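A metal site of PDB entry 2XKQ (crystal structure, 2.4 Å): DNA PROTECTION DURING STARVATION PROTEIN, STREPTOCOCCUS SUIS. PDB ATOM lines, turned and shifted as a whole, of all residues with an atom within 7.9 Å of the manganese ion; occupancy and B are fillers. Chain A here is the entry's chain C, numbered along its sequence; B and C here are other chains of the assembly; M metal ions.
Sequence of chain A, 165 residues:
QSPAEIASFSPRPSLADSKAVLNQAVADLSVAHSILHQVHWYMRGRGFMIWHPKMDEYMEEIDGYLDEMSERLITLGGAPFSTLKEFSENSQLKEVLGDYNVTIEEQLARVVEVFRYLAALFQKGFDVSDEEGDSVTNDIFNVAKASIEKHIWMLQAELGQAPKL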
ATOM      1  N   ASP A  63      15.462  14.159  12.144  1.00  0.00           N
ATOM      2  CA  ASP A  63      14.648  14.190  13.368  1.00  0.00           C
ATOM      3  C   ASP A  63      14.222  15.645  13.732  1.00  0.00           C
ATOM      4  O   ASP A  63      13.116  15.868  14.240  1.00  0.00           O
ATOM      5  CB  ASP A  63      15.361  13.497  14.568  1.00  0.00           C
ATOM      6  CG  ASP A  63      15.272  11.914  14.514  1.00  0.00           C
ATOM      7  OD1 ASP A  63      16.149  11.233  15.140  1.00  0.00           O
ATOM      8  OD2 ASP A  63      14.349  11.336  13.871  1.00  0.00           O
ATOM      9  N   LEU A  66      11.365  16.861  11.489  1.00  0.00           N
ATOM     10  CA  LEU A  66      10.208  16.093  11.875  1.00  0.00           C
ATOM     11  C   LEU A  66       9.502  16.751  13.055  1.00  0.00           C
ATOM     12  O   LEU A  66       8.302  17.048  13.015  1.00  0.00           O
ATOM     13  CB  LEU A  66      10.623  14.645  12.191  1.00  0.00           C
ATOM     14  CG  LEU A  66       9.628  13.610  12.759  1.00  0.00           C
ATOM     15  CD1 LEU A  66       8.234  13.793  12.170  1.00  0.00           C
ATOM     16  CD2 LEU A  66      10.139  12.165  12.568  1.00  0.00           C
ATOM     17  N   ASP A  67      10.264  17.020  14.102  1.00  0.00           N
ATOM     18  CA  ASP A  67       9.695  17.532  15.342  1.00  0.00           C
ATOM     19  C   ASP A  67       9.161  18.963  15.179  1.00  0.00           C
ATOM     20  O   ASP A  67       8.069  19.283  15.666  1.00  0.00           O
ATOM     21  CB  ASP A  67      10.701  17.420  16.482  1.00  0.00           C
ATOM     22  CG  ASP A  67      10.028  17.414  17.840  1.00  0.00           C
ATOM     23  OD1 ASP A  67      10.480  18.171  18.722  1.00  0.00           O
ATOM     24  OD2 ASP A  67       9.024  16.668  18.017  1.00  0.00           O
ATOM     25  N   GLU A  68       9.898  19.785  14.443  1.00  0.00           N
ATOM     26  CA  GLU A  68       9.470  21.126  14.097  1.00  0.00           C
ATOM     27  C   GLU A  68       8.167  21.124  13.266  1.00  0.00           C
ATOM     28  O   GLU A  68       7.308  21.986  13.443  1.00  0.00           O
ATOM     29  CB  GLU A  68      10.578  21.822  13.312  1.00  0.00           C
ATOM     30  CG  GLU A  68      10.510  23.325  13.343  1.00  0.00           C
ATOM     31  CD  GLU A  68      11.691  23.989  12.632  1.00  0.00           C
ATOM     32  OE1 GLU A  68      12.251  23.341  11.689  1.00  0.00           O
ATOM     33  OE2 GLU A  68      12.037  25.133  13.005  1.00  0.00           O
ATOM     34  N   SER A  70       5.757  18.572  12.894  1.00  0.00           N
ATOM     35  CA  SER A  70       4.620  18.080  13.663  1.00  0.00           C
ATOM     36  C   SER A  70       4.092  19.174  14.594  1.00  0.00           C
ATOM     37  O   SER A  70       2.875  19.461  14.624  1.00  0.00           O
ATOM     38  CB  SER A  70       5.052  16.898  14.504  1.00  0.00           C
ATOM     39  OG  SER A  70       3.924  16.262  15.084  1.00  0.00           O
ATOM     40  N   GLU A  71       5.016  19.781  15.341  1.00  0.00           N
ATOM     41  CA  GLU A  71       4.659  20.815  16.313  1.00  0.00           C
ATOM     42  C   GLU A  71       3.976  22.040  15.731  1.00  0.00           C
ATOM     43  O   GLU A  71       3.078  22.615  16.366  1.00  0.00           O
ATOM     44  CB  GLU A  71       5.859  21.186  17.151  1.00  0.00           C
ATOM     45  CG  GLU A  71       5.982  20.209  18.253  1.00  0.00           C
ATOM     46  CD  GLU A  71       7.271  20.314  19.003  1.00  0.00           C
ATOM     47  OE1 GLU A  71       7.886  21.416  19.045  1.00  0.00           O
ATOM     48  OE2 GLU A  71       7.646  19.253  19.555  1.00  0.00           O
ATOM     49  N   ILE A  74       0.388  20.826  15.137  1.00  0.00           N
ATOM     50  CA  ILE A  74      -0.336  20.957  16.409  1.00  0.00           C
ATOM     51  C   ILE A  74      -0.721  22.428  16.691  1.00  0.00           C
ATOM     52  O   ILE A  74      -1.869  22.720  17.048  1.00  0.00           O
ATOM     53  CB  ILE A  74       0.446  20.379  17.624  1.00  0.00           C
ATOM     54  CG1 ILE A  74       0.957  18.967  17.313  1.00  0.00           C
ATOM     55  CG2 ILE A  74      -0.448  20.414  18.885  1.00  0.00           C
ATOM     56  CD1 ILE A  74       1.964  18.412  18.317  1.00  0.00           C
ATOM     57  N   HIS B  37       6.547   9.464  21.499  1.00  0.00           N
ATOM     58  CA  HIS B  37       6.393  10.619  20.608  1.00  0.00           C
ATOM     59  C   HIS B  37       4.933  11.094  20.602  1.00  0.00           C
ATOM     60  O   HIS B  37       4.682  12.288  20.724  1.00  0.00           O
ATOM     61  CB  HIS B  37       6.886  10.299  19.186  1.00  0.00           C
ATOM     62  CG  HIS B  37       7.780  11.352  18.577  1.00  0.00           C
ATOM     63  ND1 HIS B  37       7.798  12.671  19.012  1.00  0.00           N
ATOM     64  CD2 HIS B  37       8.676  11.281  17.562  1.00  0.00           C
ATOM     65  CE1 HIS B  37       8.673  13.355  18.294  1.00  0.00           C
ATOM     66  NE2 HIS B  37       9.206  12.540  17.403  1.00  0.00           N
ATOM     67  N   HIS B  40       4.143  12.756  23.882  1.00  0.00           N
ATOM     68  CA  HIS B  40       4.789  14.077  23.783  1.00  0.00           C
ATOM     69  C   HIS B  40       3.935  15.071  23.002  1.00  0.00           C
ATOM     70  O   HIS B  40       3.739  16.196  23.447  1.00  0.00           O
ATOM     71  CB  HIS B  40       6.176  13.914  23.153  1.00  0.00           C
ATOM     72  CG  HIS B  40       6.952  15.171  22.958  1.00  0.00           C
ATOM     73  ND1 HIS B  40       7.751  15.710  23.947  1.00  0.00           N
ATOM     74  CD2 HIS B  40       7.150  15.943  21.860  1.00  0.00           C
ATOM     75  CE1 HIS B  40       8.368  16.783  23.476  1.00  0.00           C
ATOM     76  NE2 HIS B  40       8.012  16.947  22.219  1.00  0.00           N
ATOM     77  N   TRP B  41       3.413  14.670  21.846  1.00  0.00           N
ATOM     78  CA  TRP B  41       2.638  15.611  21.016  1.00  0.00           C
ATOM     79  C   TRP B  41       1.210  15.927  21.524  1.00  0.00           C
ATOM     80  O   TRP B  41       0.805  17.097  21.502  1.00  0.00           O
ATOM     81  CB  TRP B  41       2.554  15.116  19.572  1.00  0.00           C
ATOM     82  CG  TRP B  41       3.850  15.184  18.798  1.00  0.00           C
ATOM     83  CD1 TRP B  41       4.863  16.110  18.923  1.00  0.00           C
ATOM     84  CD2 TRP B  41       4.232  14.329  17.700  1.00  0.00           C
ATOM     85  NE1 TRP B  41       5.839  15.863  17.984  1.00  0.00           N
ATOM     86  CE2 TRP B  41       5.490  14.771  17.235  1.00  0.00           C
ATOM     87  CE3 TRP B  41       3.626  13.219  17.078  1.00  0.00           C
ATOM     88  CZ2 TRP B  41       6.159  14.151  16.188  1.00  0.00           C
ATOM     89  CZ3 TRP B  41       4.317  12.583  16.017  1.00  0.00           C
ATOM     90  CH2 TRP B  41       5.570  13.061  15.592  1.00  0.00           C
ATOM     91  N   HIS B  52       6.083  17.270  29.267  1.00  0.00           N
ATOM     92  CA  HIS B  52       6.317  17.405  27.805  1.00  0.00           C
ATOM     93  C   HIS B  52       7.820  17.237  27.431  1.00  0.00           C
ATOM     94  O   HIS B  52       8.131  16.294  26.692  1.00  0.00           O
ATOM     95  CB  HIS B  52       5.646  18.660  27.182  1.00  0.00           C
ATOM     96  CG  HIS B  52       6.053  18.969  25.756  1.00  0.00           C
ATOM     97  ND1 HIS B  52       5.448  18.364  24.654  1.00  0.00           N
ATOM     98  CD2 HIS B  52       6.966  19.829  25.255  1.00  0.00           C
ATOM     99  CE1 HIS B  52       5.993  18.838  23.545  1.00  0.00           C
ATOM    100  NE2 HIS B  52       6.913  19.733  23.880  1.00  0.00           N
ATOM    101  N   PRO B  53       8.728  18.088  27.980  1.00  0.00           N
ATOM    102  CA  PRO B  53      10.180  17.869  27.716  1.00  0.00           C
ATOM    103  C   PRO B  53      10.728  16.567  28.318  1.00  0.00           C
ATOM    104  O   PRO B  53      11.705  16.028  27.800  1.00  0.00           O
ATOM    105  CB  PRO B  53      10.888  19.091  28.338  1.00  0.00           C
ATOM    106  CG  PRO B  53       9.890  19.660  29.319  1.00  0.00           C
ATOM    107  CD  PRO B  53       8.490  19.262  28.845  1.00  0.00           C
ATOM    108  N   ASP B  56      10.947  13.749  25.858  1.00  0.00           N
ATOM    109  CA  ASP B  56      12.203  13.902  25.112  1.00  0.00           C
ATOM    110  C   ASP B  56      13.390  13.106  25.689  1.00  0.00           C
ATOM    111  O   ASP B  56      14.086  12.422  24.948  1.00  0.00           O
ATOM    112  CB  ASP B  56      12.614  15.379  24.977  1.00  0.00           C
ATOM    113  CG  ASP B  56      12.155  15.992  23.672  1.00  0.00           C
ATOM    114  OD1 ASP B  56      11.589  17.112  23.708  1.00  0.00           O
ATOM    115  OD2 ASP B  56      12.369  15.353  22.628  1.00  0.00           O
ATOM    116  N   MET B  59      12.710   9.361  25.121  1.00  0.00           N
ATOM    117  CA  MET B  59      12.977   8.965  23.716  1.00  0.00           C
ATOM    118  C   MET B  59      14.474   8.798  23.364  1.00  0.00           C
ATOM    119  O   MET B  59      14.838   7.911  22.598  1.00  0.00           O
ATOM    120  CB  MET B  59      12.303   9.929  22.720  1.00  0.00           C
ATOM    121  CG  MET B  59      10.833   9.640  22.460  1.00  0.00           C
ATOM    122  SD  MET B  59      10.145  10.802  21.246  1.00  0.00           S
ATOM    123  CE  MET B  59       9.814  12.262  22.274  1.00  0.00           C
ATOM    124  N   LYS C 150       4.172  29.318  19.109  1.00  0.00           N
ATOM    125  CA  LYS C 150       4.625  28.102  19.758  1.00  0.00           C
ATOM    126  C   LYS C 150       4.375  28.153  21.269  1.00  0.00           C
ATOM    127  O   LYS C 150       3.917  27.167  21.846  1.00  0.00           O
ATOM    128  CB  LYS C 150       6.099  27.866  19.436  1.00  0.00           C
ATOM    129  CG  LYS C 150       6.632  26.484  19.757  1.00  0.00           C
ATOM    130  CD  LYS C 150       8.163  26.361  19.548  1.00  0.00           C
ATOM    131  CE  LYS C 150       8.574  25.883  18.111  1.00  0.00           C
ATOM    132  NZ  LYS C 150       8.421  24.374  17.870  1.00  0.00           N
ATOM    133  N   TRP C 153       0.508  27.588  22.058  1.00  0.00           N
ATOM    134  CA  TRP C 153       0.242  26.141  22.110  1.00  0.00           C
ATOM    135  C   TRP C 153       0.548  25.530  23.499  1.00  0.00           C
ATOM    136  O   TRP C 153      -0.333  24.917  24.134  1.00  0.00           O
ATOM    137  CB  TRP C 153       1.005  25.375  20.998  1.00  0.00           C
ATOM    138  CG  TRP C 153       1.288  23.909  21.349  1.00  0.00           C
ATOM    139  CD1 TRP C 153       0.392  22.998  21.842  1.00  0.00           C
ATOM    140  CD2 TRP C 153       2.542  23.208  21.217  1.00  0.00           C
ATOM    141  NE1 TRP C 153       1.011  21.784  22.038  1.00  0.00           N
ATOM    142  CE2 TRP C 153       2.320  21.886  21.668  1.00  0.00           C
ATOM    143  CE3 TRP C 153       3.819  23.581  20.783  1.00  0.00           C
ATOM    144  CZ2 TRP C 153       3.350  20.922  21.694  1.00  0.00           C
ATOM    145  CZ3 TRP C 153       4.830  22.619  20.804  1.00  0.00           C
ATOM    146  CH2 TRP C 153       4.595  21.312  21.270  1.00  0.00           C
ATOM    147  N   MET C 154       1.786  25.710  23.964  1.00  0.00           N
ATOM    148  CA  MET C 154       2.237  25.146  25.232  1.00  0.00           C
ATOM    149  C   MET C 154       1.426  25.689  26.421  1.00  0.00           C
ATOM    150  O   MET C 154       1.020  24.905  27.299  1.00  0.00           O
ATOM    151  CB  MET C 154       3.742  25.350  25.440  1.00  0.00           C
ATOM    152  CG  MET C 154       4.656  24.572  24.431  1.00  0.00           C
ATOM    153  SD  MET C 154       6.377  24.529  24.991  1.00  0.00           S
ATOM    154  CE  MET C 154       7.170  23.471  23.774  1.00  0.00           C
HETATM  155 MN    MN M   1       9.171  18.135  20.507  1.00  0.00          MN
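The side-chain carboxylate (OE1) of Glu 71 is in salt-bridge range of the side-chain amino group (NZ) of Lys 150 of chain C, 3.2 Å away. OD2 of Asp 67 sits at hydrogen-bond distance from NE1 of Trp 41 of chain B (3.3 Å). ND1 of His 40 of chain B is in hydrogen-bond range of O of His 52 of chain B, 2.8 Å away.
OE2 of Glu 71 binds the manganese ion (2.1 Å). OD1 of Asp 67 binds the manganese ion (2.2 Å). NE2 of His 40 of chain B binds the manganese ion (2.4 Å). Slightly farther from the manganese ion lies the side-chain carboxylate (OD2) of Asp 67 (2.9 Å).
Of the 17 residues printed, 3 come within 4 Å of the manganese ion. The nearest printed residue that does not touch the manganese ion is Asp 56 of chain B (4.1 Å).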
